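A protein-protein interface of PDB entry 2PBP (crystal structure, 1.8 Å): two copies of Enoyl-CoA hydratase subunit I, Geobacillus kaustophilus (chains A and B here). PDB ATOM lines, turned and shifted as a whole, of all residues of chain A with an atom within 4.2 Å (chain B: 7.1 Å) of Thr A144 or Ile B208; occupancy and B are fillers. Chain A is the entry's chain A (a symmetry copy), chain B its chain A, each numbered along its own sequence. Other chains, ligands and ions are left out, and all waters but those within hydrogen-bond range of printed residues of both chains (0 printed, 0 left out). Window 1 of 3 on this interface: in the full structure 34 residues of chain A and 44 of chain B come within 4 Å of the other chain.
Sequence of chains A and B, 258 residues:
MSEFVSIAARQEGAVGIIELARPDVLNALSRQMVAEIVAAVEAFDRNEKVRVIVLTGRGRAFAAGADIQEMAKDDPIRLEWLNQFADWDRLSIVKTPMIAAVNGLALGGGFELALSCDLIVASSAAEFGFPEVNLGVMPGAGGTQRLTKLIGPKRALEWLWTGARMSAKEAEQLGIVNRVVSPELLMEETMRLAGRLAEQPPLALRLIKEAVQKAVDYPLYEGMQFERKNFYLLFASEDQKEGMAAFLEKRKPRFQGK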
ATOM      1  N   MET A 138      -9.315  23.355 -21.670  1.00  0.00           N
ATOM      2  CA  MET A 138      -8.228  24.130 -21.070  1.00  0.00           C
ATOM      3  C   MET A 138      -8.738  25.397 -20.384  1.00  0.00           C
ATOM      4  O   MET A 138      -9.917  25.734 -20.481  1.00  0.00           O
ATOM      5  CB  MET A 138      -7.227  24.532 -22.161  1.00  0.00           C
ATOM      6  CG  MET A 138      -7.785  25.504 -23.203  1.00  0.00           C
ATOM      7  SD  MET A 138      -6.628  25.895 -24.548  1.00  0.00           S
ATOM      8  CE  MET A 138      -5.663  27.230 -23.807  1.00  0.00           C
ATOM      9  N   PRO A 139      -7.853  26.106 -19.662  1.00  0.00           N
ATOM     10  CA  PRO A 139      -8.296  27.338 -19.003  1.00  0.00           C
ATOM     11  C   PRO A 139      -8.540  28.360 -20.115  1.00  0.00           C
ATOM     12  O   PRO A 139      -7.759  28.446 -21.059  1.00  0.00           O
ATOM     13  CB  PRO A 139      -7.103  27.708 -18.129  1.00  0.00           C
ATOM     14  CG  PRO A 139      -6.521  26.360 -17.776  1.00  0.00           C
ATOM     15  CD  PRO A 139      -6.562  25.651 -19.111  1.00  0.00           C
ATOM     16  N   GLY A 142      -7.572  33.476 -18.812  1.00  0.00           N
ATOM     17  CA  GLY A 142      -6.296  33.999 -18.359  1.00  0.00           C
ATOM     18  C   GLY A 142      -5.406  33.053 -17.575  1.00  0.00           C
ATOM     19  O   GLY A 142      -4.242  33.363 -17.328  1.00  0.00           O
ATOM     20  N   GLY A 143      -5.947  31.906 -17.178  1.00  0.00           N
ATOM     21  CA  GLY A 143      -5.174  30.942 -16.415  1.00  0.00           C
ATOM     22  C   GLY A 143      -3.816  30.587 -17.000  1.00  0.00           C
ATOM     23  O   GLY A 143      -2.810  30.607 -16.290  1.00  0.00           O
ATOM     24  N   THR A 144      -3.770  30.261 -18.290  1.00  0.00           N
ATOM     25  CA  THR A 144      -2.502  29.893 -18.913  1.00  0.00           C
ATOM     26  C   THR A 144      -1.555  31.083 -19.006  1.00  0.00           C
ATOM     27  O   THR A 144      -0.335  30.919 -18.973  1.00  0.00           O
ATOM     28  CB  THR A 144      -2.696  29.323 -20.337  1.00  0.00           C
ATOM     29  OG1 THR A 144      -3.195  30.347 -21.206  1.00  0.00           O
ATOM     30  CG2 THR A 144      -3.666  28.159 -20.318  1.00  0.00           C
ATOM     31  N   GLN A 145      -2.119  32.282 -19.111  1.00  0.00           N
ATOM     32  CA  GLN A 145      -1.311  33.489 -19.232  1.00  0.00           C
ATOM     33  C   GLN A 145      -0.745  33.976 -17.906  1.00  0.00           C
ATOM     34  O   GLN A 145       0.471  34.123 -17.756  1.00  0.00           O
ATOM     35  CB  GLN A 145      -2.134  34.608 -19.874  1.00  0.00           C
ATOM     36  CG  GLN A 145      -2.723  34.247 -21.234  1.00  0.00           C
ATOM     37  CD  GLN A 145      -1.668  33.767 -22.212  1.00  0.00           C
ATOM     38  OE1 GLN A 145      -1.627  32.586 -22.572  1.00  0.00           O
ATOM     39  NE2 GLN A 145      -0.799  34.675 -22.638  1.00  0.00           N
ATOM     40  N   ARG A 146      -1.624  34.228 -16.943  1.00  0.00           N
ATOM     41  CA  ARG A 146      -1.180  34.719 -15.647  1.00  0.00           C
ATOM     42  C   ARG A 146      -0.275  33.745 -14.900  1.00  0.00           C
ATOM     43  O   ARG A 146       0.694  34.168 -14.267  1.00  0.00           O
ATOM     44  CB  ARG A 146      -2.385  35.104 -14.783  1.00  0.00           C
ATOM     45  CG  ARG A 146      -3.149  36.330 -15.299  1.00  0.00           C
ATOM     46  CD  ARG A 146      -4.075  36.893 -14.225  1.00  0.00           C
ATOM     47  NE  ARG A 146      -4.633  38.198 -14.579  1.00  0.00           N
ATOM     48  CZ  ARG A 146      -5.787  38.383 -15.214  1.00  0.00           C
ATOM     49  NH1 ARG A 146      -6.530  37.345 -15.578  1.00  0.00           N
ATOM     50  NH2 ARG A 146      -6.202  39.615 -15.484  1.00  0.00           N
ATOM     51  N   THR A 148       1.777  31.457 -16.196  1.00  0.00           N
ATOM     52  CA  THR A 148       3.071  31.429 -16.869  1.00  0.00           C
ATOM     53  C   THR A 148       3.913  32.664 -16.546  1.00  0.00           C
ATOM     54  O   THR A 148       5.123  32.566 -16.338  1.00  0.00           O
ATOM     55  CB  THR A 148       2.894  31.318 -18.397  1.00  0.00           C
ATOM     56  OG1 THR A 148       2.217  30.091 -18.705  1.00  0.00           O
ATOM     57  CG2 THR A 148       4.250  31.330 -19.098  1.00  0.00           C
ATOM     58  N   LEU A 157       3.577  24.641 -17.289  1.00  0.00           N
ATOM     59  CA  LEU A 157       3.109  23.515 -18.095  1.00  0.00           C
ATOM     60  C   LEU A 157       2.881  22.263 -17.260  1.00  0.00           C
ATOM     61  O   LEU A 157       1.989  21.468 -17.553  1.00  0.00           O
ATOM     62  CB  LEU A 157       4.086  23.232 -19.239  1.00  0.00           C
ATOM     63  CG  LEU A 157       4.011  24.259 -20.377  1.00  0.00           C
ATOM     64  CD1 LEU A 157       5.115  24.002 -21.391  1.00  0.00           C
ATOM     65  CD2 LEU A 157       2.632  24.180 -21.039  1.00  0.00           C
ATOM     66  N   LEU A 160      -0.543  22.946 -15.680  1.00  0.00           N
ATOM     67  CA  LEU A 160      -1.585  23.042 -16.697  1.00  0.00           C
ATOM     68  C   LEU A 160      -1.839  21.724 -17.429  1.00  0.00           C
ATOM     69  O   LEU A 160      -2.985  21.395 -17.734  1.00  0.00           O
ATOM     70  CB  LEU A 160      -1.223  24.142 -17.703  1.00  0.00           C
ATOM     71  CG  LEU A 160      -1.191  25.559 -17.117  1.00  0.00           C
ATOM     72  CD1 LEU A 160      -0.492  26.508 -18.078  1.00  0.00           C
ATOM     73  CD2 LEU A 160      -2.621  26.025 -16.837  1.00  0.00           C
ATOM     74  N   TRP A 161      -0.777  20.971 -17.698  1.00  0.00           N
ATOM     75  CA  TRP A 161      -0.906  19.695 -18.401  1.00  0.00           C
ATOM     76  C   TRP A 161      -1.453  18.551 -17.541  1.00  0.00           C
ATOM     77  O   TRP A 161      -2.144  17.668 -18.050  1.00  0.00           O
ATOM     78  CB  TRP A 161       0.445  19.264 -18.976  1.00  0.00           C
ATOM     79  CG  TRP A 161       0.845  19.931 -20.263  1.00  0.00           C
ATOM     80  CD1 TRP A 161       0.061  20.701 -21.080  1.00  0.00           C
ATOM     81  CD2 TRP A 161       2.110  19.813 -20.916  1.00  0.00           C
ATOM     82  NE1 TRP A 161       0.763  21.064 -22.206  1.00  0.00           N
ATOM     83  CE2 TRP A 161       2.026  20.531 -22.132  1.00  0.00           C
ATOM     84  CE3 TRP A 161       3.312  19.163 -20.598  1.00  0.00           C
ATOM     85  CZ2 TRP A 161       3.096  20.620 -23.027  1.00  0.00           C
ATOM     86  CZ3 TRP A 161       4.377  19.251 -21.486  1.00  0.00           C
ATOM     87  CH2 TRP A 161       4.260  19.974 -22.689  1.00  0.00           C
ATOM     88  N   PRO B 202      -4.478  14.904 -26.285  1.00  0.00           N
ATOM     89  CA  PRO B 202      -3.411  15.458 -27.130  1.00  0.00           C
ATOM     90  C   PRO B 202      -3.654  16.896 -27.604  1.00  0.00           C
ATOM     91  O   PRO B 202      -2.736  17.723 -27.593  1.00  0.00           O
ATOM     92  CB  PRO B 202      -3.342  14.465 -28.291  1.00  0.00           C
ATOM     93  CG  PRO B 202      -3.740  13.164 -27.644  1.00  0.00           C
ATOM     94  CD  PRO B 202      -4.925  13.596 -26.792  1.00  0.00           C
ATOM     95  N   LEU B 203      -4.883  17.192 -28.020  1.00  0.00           N
ATOM     96  CA  LEU B 203      -5.215  18.534 -28.497  1.00  0.00           C
ATOM     97  C   LEU B 203      -5.146  19.540 -27.353  1.00  0.00           C
ATOM     98  O   LEU B 203      -4.714  20.680 -27.541  1.00  0.00           O
ATOM     99  CB  LEU B 203      -6.611  18.547 -29.130  1.00  0.00           C
ATOM    100  CG  LEU B 203      -6.733  17.789 -30.454  1.00  0.00           C
ATOM    101  CD1 LEU B 203      -8.196  17.474 -30.737  1.00  0.00           C
ATOM    102  CD2 LEU B 203      -6.121  18.616 -31.581  1.00  0.00           C
ATOM    103  N   ALA B 204      -5.567  19.117 -26.165  1.00  0.00           N
ATOM    104  CA  ALA B 204      -5.520  20.000 -25.008  1.00  0.00           C
ATOM    105  C   ALA B 204      -4.065  20.311 -24.653  1.00  0.00           C
ATOM    106  O   ALA B 204      -3.722  21.468 -24.415  1.00  0.00           O
ATOM    107  CB  ALA B 204      -6.244  19.362 -23.816  1.00  0.00           C
ATOM    108  N   LEU B 205      -3.199  19.297 -24.620  1.00  0.00           N
ATOM    109  CA  LEU B 205      -1.795  19.554 -24.291  1.00  0.00           C
ATOM    110  C   LEU B 205      -1.146  20.463 -25.339  1.00  0.00           C
ATOM    111  O   LEU B 205      -0.368  21.359 -25.011  1.00  0.00           O
ATOM    112  CB  LEU B 205      -0.998  18.248 -24.193  1.00  0.00           C
ATOM    113  CG  LEU B 205      -1.401  17.224 -23.129  1.00  0.00           C
ATOM    114  CD1 LEU B 205      -0.237  16.261 -22.897  1.00  0.00           C
ATOM    115  CD2 LEU B 205      -1.765  17.922 -21.830  1.00  0.00           C
ATOM    116  N   ARG B 206      -1.487  20.228 -26.601  1.00  0.00           N
ATOM    117  CA  ARG B 206      -0.957  20.992 -27.724  1.00  0.00           C
ATOM    118  C   ARG B 206      -1.359  22.465 -27.662  1.00  0.00           C
ATOM    119  O   ARG B 206      -0.510  23.353 -27.763  1.00  0.00           O
ATOM    120  CB  ARG B 206      -1.459  20.373 -29.031  1.00  0.00           C
ATOM    121  CG  ARG B 206      -1.015  21.050 -30.328  1.00  0.00           C
ATOM    122  CD  ARG B 206      -1.851  20.471 -31.469  1.00  0.00           C
ATOM    123  NE  ARG B 206      -1.521  20.964 -32.805  1.00  0.00           N
ATOM    124  CZ  ARG B 206      -0.525  20.502 -33.553  1.00  0.00           C
ATOM    125  NH1 ARG B 206       0.261  19.534 -33.098  1.00  0.00           N
ATOM    126  NH2 ARG B 206      -0.344  20.974 -34.783  1.00  0.00           N
ATOM    127  N   LEU B 207      -2.652  22.720 -27.494  1.00  0.00           N
ATOM    128  CA  LEU B 207      -3.148  24.091 -27.441  1.00  0.00           C
ATOM    129  C   LEU B 207      -2.779  24.822 -26.152  1.00  0.00           C
ATOM    130  O   LEU B 207      -2.657  26.048 -26.143  1.00  0.00           O
ATOM    131  CB  LEU B 207      -4.662  24.113 -27.678  1.00  0.00           C
ATOM    132  CG  LEU B 207      -5.050  24.142 -29.169  1.00  0.00           C
ATOM    133  CD1 LEU B 207      -4.340  23.019 -29.921  1.00  0.00           C
ATOM    134  CD2 LEU B 207      -6.561  24.023 -29.321  1.00  0.00           C
ATOM    135  N   ILE B 208      -2.606  24.078 -25.063  1.00  0.00           N
ATOM    136  CA  ILE B 208      -2.202  24.695 -23.802  1.00  0.00           C
ATOM    137  C   ILE B 208      -0.764  25.175 -23.982  1.00  0.00           C
ATOM    138  O   ILE B 208      -0.402  26.283 -23.574  1.00  0.00           O
ATOM    139  CB  ILE B 208      -2.250  23.688 -22.618  1.00  0.00           C
ATOM    140  CG1 ILE B 208      -3.687  23.550 -22.107  1.00  0.00           C
ATOM    141  CG2 ILE B 208      -1.309  24.149 -21.505  1.00  0.00           C
ATOM    142  CD1 ILE B 208      -4.372  24.826 -21.549  1.00  0.00           C
ATOM    143  N   LYS B 209       0.052  24.323 -24.593  1.00  0.00           N
ATOM    144  CA  LYS B 209       1.446  24.652 -24.836  1.00  0.00           C
ATOM    145  C   LYS B 209       1.546  25.904 -25.710  1.00  0.00           C
ATOM    146  O   LYS B 209       2.370  26.782 -25.447  1.00  0.00           O
ATOM    147  CB  LYS B 209       2.157  23.470 -25.507  1.00  0.00           C
ATOM    148  CG  LYS B 209       3.589  23.765 -25.923  1.00  0.00           C
ATOM    149  CD  LYS B 209       4.296  22.511 -26.425  1.00  0.00           C
ATOM    150  CE  LYS B 209       5.618  22.873 -27.079  1.00  0.00           C
ATOM    151  NZ  LYS B 209       6.412  21.666 -27.459  1.00  0.00           N
ATOM    152  N   GLU B 210       0.712  25.991 -26.745  1.00  0.00           N
ATOM    153  CA  GLU B 210       0.734  27.160 -27.622  1.00  0.00           C
ATOM    154  C   GLU B 210       0.407  28.417 -26.829  1.00  0.00           C
ATOM    155  O   GLU B 210       1.045  29.455 -27.001  1.00  0.00           O
ATOM    156  CB  GLU B 210      -0.287  27.033 -28.753  1.00  0.00           C
ATOM    157  CG  GLU B 210      -0.043  25.911 -29.728  1.00  0.00           C
ATOM    158  CD  GLU B 210      -1.001  25.981 -30.901  1.00  0.00           C
ATOM    159  OE1 GLU B 210      -2.190  26.290 -30.671  1.00  0.00           O
ATOM    160  OE2 GLU B 210      -0.570  25.728 -32.045  1.00  0.00           O
ATOM    161  N   ALA B 211      -0.603  28.320 -25.970  1.00  0.00           N
ATOM    162  CA  ALA B 211      -1.013  29.458 -25.156  1.00  0.00           C
ATOM    163  C   ALA B 211       0.119  29.878 -24.222  1.00  0.00           C
ATOM    164  O   ALA B 211       0.393  31.066 -24.062  1.00  0.00           O
ATOM    165  CB  ALA B 211      -2.262  29.106 -24.350  1.00  0.00           C
ATOM    166  N   VAL B 212       0.779  28.900 -23.606  1.00  0.00           N
ATOM    167  CA  VAL B 212       1.879  29.201 -22.701  1.00  0.00           C
ATOM    168  C   VAL B 212       3.026  29.876 -23.450  1.00  0.00           C
ATOM    169  O   VAL B 212       3.683  30.767 -22.915  1.00  0.00           O
ATOM    170  CB  VAL B 212       2.392  27.920 -22.000  1.00  0.00           C
ATOM    171  CG1 VAL B 212       3.680  28.212 -21.240  1.00  0.00           C
ATOM    172  CG2 VAL B 212       1.330  27.406 -21.045  1.00  0.00           C
ATOM    173  N   GLN B 213       3.258  29.461 -24.693  1.00  0.00           N
ATOM    174  CA  GLN B 213       4.325  30.050 -25.494  1.00  0.00           C
ATOM    175  C   GLN B 213       4.042  31.543 -25.682  1.00  0.00           C
ATOM    176  O   GLN B 213       4.954  32.365 -25.633  1.00  0.00           O
ATOM    177  CB  GLN B 213       4.419  29.382 -26.873  1.00  0.00           C
ATOM    178  CG  GLN B 213       4.463  27.853 -26.883  1.00  0.00           C
ATOM    179  CD  GLN B 213       5.548  27.258 -25.999  1.00  0.00           C
ATOM    180  OE1 GLN B 213       5.345  27.046 -24.800  1.00  0.00           O
ATOM    181  NE2 GLN B 213       6.708  26.984 -26.589  1.00  0.00           N
ATOM    182  N   LYS B 214       2.776  31.887 -25.896  1.00  0.00           N
ATOM    183  CA  LYS B 214       2.390  33.283 -26.081  1.00  0.00           C
ATOM    184  C   LYS B 214       2.502  34.049 -24.760  1.00  0.00           C
ATOM    185  O   LYS B 214       2.887  35.217 -24.745  1.00  0.00           O
ATOM    186  CB  LYS B 214       0.950  33.382 -26.603  1.00  0.00           C
ATOM    187  CG  LYS B 214       0.629  32.477 -27.796  1.00  0.00           C
ATOM    188  CD  LYS B 214       1.586  32.697 -28.959  1.00  0.00           C
ATOM    189  CE  LYS B 214       1.204  31.836 -30.159  1.00  0.00           C
ATOM    190  NZ  LYS B 214       2.245  31.885 -31.224  1.00  0.00           N
ATOM    191  N   ALA B 215       2.171  33.382 -23.655  1.00  0.00           N
ATOM    192  CA  ALA B 215       2.224  34.003 -22.331  1.00  0.00           C
ATOM    193  C   ALA B 215       3.617  34.509 -21.986  1.00  0.00           C
ATOM    194  O   ALA B 215       3.771  35.476 -21.241  1.00  0.00           O
ATOM    195  CB  ALA B 215       1.756  33.013 -21.270  1.00  0.00           C
ATOM    196  N   VAL B 216       4.632  33.844 -22.523  1.00  0.00           N
ATOM    197  CA  VAL B 216       6.015  34.231 -22.272  1.00  0.00           C
ATOM    198  C   VAL B 216       6.378  35.539 -22.980  1.00  0.00           C
ATOM    199  O   VAL B 216       7.191  36.316 -22.476  1.00  0.00           O
ATOM    200  CB  VAL B 216       6.994  33.122 -22.744  1.00  0.00           C
ATOM    201  CG1 VAL B 216       8.432  33.600 -22.624  1.00  0.00           C
ATOM    202  CG2 VAL B 216       6.795  31.860 -21.909  1.00  0.00           C
ATOM    203  N   GLY B 223      -2.568  37.931 -24.953  1.00  0.00           N
ATOM    204  CA  GLY B 223      -2.279  36.531 -24.697  1.00  0.00           C
ATOM    205  C   GLY B 223      -3.591  35.827 -24.392  1.00  0.00           C
ATOM    206  O   GLY B 223      -3.814  34.684 -24.795  1.00  0.00           O
ATOM    207  N   MET B 224      -4.468  36.524 -23.677  1.00  0.00           N
ATOM    208  CA  MET B 224      -5.774  35.979 -23.329  1.00  0.00           C
ATOM    209  C   MET B 224      -6.669  35.909 -24.568  1.00  0.00           C
ATOM    210  O   MET B 224      -7.510  35.018 -24.685  1.00  0.00           O
ATOM    211  CB  MET B 224      -6.419  36.831 -22.227  1.00  0.00           C
ATOM    212  CG  MET B 224      -5.772  36.595 -20.856  1.00  0.00           C
ATOM    213  SD  MET B 224      -6.381  37.664 -19.536  1.00  0.00           S
ATOM    214  CE  MET B 224      -8.054  37.059 -19.386  1.00  0.00           C
ATOM    215  N   GLU B 227      -5.526  32.787 -26.172  1.00  0.00           N
ATOM    216  CA  GLU B 227      -5.912  31.687 -25.300  1.00  0.00           C
ATOM    217  C   GLU B 227      -7.361  31.237 -25.511  1.00  0.00           C
ATOM    218  O   GLU B 227      -7.630  30.045 -25.698  1.00  0.00           O
ATOM    219  CB  GLU B 227      -5.713  32.114 -23.847  1.00  0.00           C
ATOM    220  CG  GLU B 227      -6.067  31.065 -22.810  1.00  0.00           C
ATOM    221  CD  GLU B 227      -6.157  31.678 -21.428  1.00  0.00           C
ATOM    222  OE1 GLU B 227      -7.016  32.562 -21.247  1.00  0.00           O
ATOM    223  OE2 GLU B 227      -5.373  31.290 -20.532  1.00  0.00           O
ATOM    224  N   ARG B 228      -8.294  32.184 -25.491  1.00  0.00           N
ATOM    225  CA  ARG B 228      -9.704  31.842 -25.658  1.00  0.00           C
ATOM    226  C   ARG B 228     -10.043  31.259 -27.030  1.00  0.00           C
ATOM    227  O   ARG B 228     -11.008  30.500 -27.155  1.00  0.00           O
ATOM    228  CB  ARG B 228     -10.594  33.055 -25.346  1.00  0.00           C
ATOM    229  CG  ARG B 228     -10.445  34.241 -26.280  1.00  0.00           C
ATOM    230  CD  ARG B 228     -11.087  35.488 -25.677  1.00  0.00           C
ATOM    231  NE  ARG B 228     -10.443  35.861 -24.420  1.00  0.00           N
ATOM    232  CZ  ARG B 228     -10.686  36.983 -23.747  1.00  0.00           C
ATOM    233  NH1 ARG B 228     -11.568  37.865 -24.206  1.00  0.00           N
ATOM    234  NH2 ARG B 228     -10.046  37.222 -22.608  1.00  0.00           N
ATOM    235  N   ASN B 230      -8.152  29.180 -28.637  1.00  0.00           N
ATOM    236  CA  ASN B 230      -7.806  27.769 -28.497  1.00  0.00           C
ATOM    237  C   ASN B 230      -8.870  27.081 -27.645  1.00  0.00           C
ATOM    238  O   ASN B 230      -9.203  25.920 -27.877  1.00  0.00           O
ATOM    239  CB  ASN B 230      -6.410  27.601 -27.876  1.00  0.00           C
ATOM    240  CG  ASN B 230      -5.305  27.596 -28.928  1.00  0.00           C
ATOM    241  OD1 ASN B 230      -5.578  27.724 -30.123  1.00  0.00           O
ATOM    242  ND2 ASN B 230      -4.055  27.440 -28.490  1.00  0.00           N
ATOM    243  N   LEU B 234     -11.101  23.714 -28.850  1.00  0.00           N
ATOM    244  CA  LEU B 234     -11.169  22.422 -28.183  1.00  0.00           C
ATOM    245  C   LEU B 234     -12.597  21.886 -28.116  1.00  0.00           C
ATOM    246  O   LEU B 234     -12.801  20.681 -27.982  1.00  0.00           O
ATOM    247  CB  LEU B 234     -10.544  22.503 -26.785  1.00  0.00           C
ATOM    248  CG  LEU B 234      -9.015  22.654 -26.797  1.00  0.00           C
ATOM    249  CD1 LEU B 234      -8.496  22.772 -25.372  1.00  0.00           C
ATOM    250  CD2 LEU B 234      -8.372  21.448 -27.489  1.00  0.00           C
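Of the 11 printed residues of chain A, 11 touch a printed residue of chain B. Printed residues of chain A that touch a printed residue of chain B: Met A138, Pro A139, Gly A142, Gly A143, Thr A144, Gln A145, Arg A146, Thr A148, Leu A157, Leu A160 and Trp A161. Among the printed residues, 32 pairs touch across the chains. Among the printed residues, no Asp or Glu carboxylate lies within 4 Å of a Lys or Arg side-chain nitrogen of the other chain.
Gly A143 touches one residue of chain B. Thr A144 touches just these residues of chain B: Ile B208 (3.6 Å), Ala B211 (3.5 Å), Ala B215 (3.7 Å) and Glu B227 (2.5 Å). Printed residues of chain B within 4 Å of Leu A157: Ile B208 (3.97 Å) and Val B212 (3.5 Å). Pro B202 touches none of the printed residues of chain A. Of chain A, only Met A138, Pro A139, Thr A144, Leu A157, Leu A160 and Trp A161 come within 4 Å of Ile B208. Of the printed residues of chain A, Val B212 touches Thr A148, Leu A157 and Leu A160. Gln B213 touches none of the printed residues of chain A. Of the printed residues of chain A, Asn B230 touches Met A138 (3.7 Å). The nearest printed residue of chain A that does not touch Ile B208 is Gln A145 (6.5 Å). The nearest printed residue of chain A that does not touch Leu B205 is Leu A160 (5.5 Å).
Among the printed residues, pairs that only touch across the chains: Met A138 with Ile B208, Gln A145 with Gly B223, Pro A139 with Ile B208, Thr A148 with Val B212, Leu A157 with Val B212, Thr A144 with Ala B211, Thr A148 with Ala B215, Met A138 with Leu B234, Pro A139 with Glu B227, Leu A160 with Val B212, Thr A144 with Ile B208, Gly A142 with Met B224, Gln A145 with Glu B227, Trp A161 with Ile B208, Thr A144 with Ala B215, Met A138 with Asn B230, Gln A145 with Met B224, Leu A160 with Ile B208, Thr A148 with Val B216, Trp A161 with Lys B209, Met A138 with Glu B227, Met A138 with Ala B211, Leu A157 with Ile B208, Arg A146 with Met B224, Gln A145 with Lys B214 and Met A138 with Leu B207.
O of Leu B205 is in hydrogen-bond range of NE1 of Trp A161. The backbone carbonyl oxygen (O) of Ala B211 lies close to the side-chain amide oxygen (OE1) of Gln A145 (2.9 Å). N of Ala B215 sits close to NE2 of Gln A145, 3.4 Å away. The side-chain carboxylate of Glu B227 lies within hydrogen-bond range of the backbone NH of Gly A142 (2.7 Å). The side-chain carboxylate (OE2) of Glu B227 lies within hydrogen-bond range of the backbone NH (N) of Gly A143 (3.5 Å). The side-chain carboxylate (OE2) of Glu B227 is in hydrogen-bond range of the side-chain hydroxyl (OG1) of Thr A144 (2.5 Å).
No position is printed for both chains. Of the 32 pairs that touch across the chains among the printed residues, none has its exchanged pair printed and touching as well.
O of Leu B207 is in hydrogen-bond range of ND2 of Asn B230 (3.1 Å). The backbone carbonyl oxygen (O) of Lys B209 sits close to the side-chain amide oxygen (OE1) of Gln B213 (3.1 Å). OE1 of Glu B210 sits at hydrogen-bond distance from ND2 of Asn B230. O of Met B224 sits at hydrogen-bond distance from NE of Arg B228, 3.1 Å away. The side-chain amide oxygen (OE1) of Gln A145 lies within hydrogen-bond range of the side-chain hydroxyl (OG1) of Thr A144 (3.1 Å). OG1 of Thr A148 lies within hydrogen-bond range of O of Thr A144 (2.7 Å).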
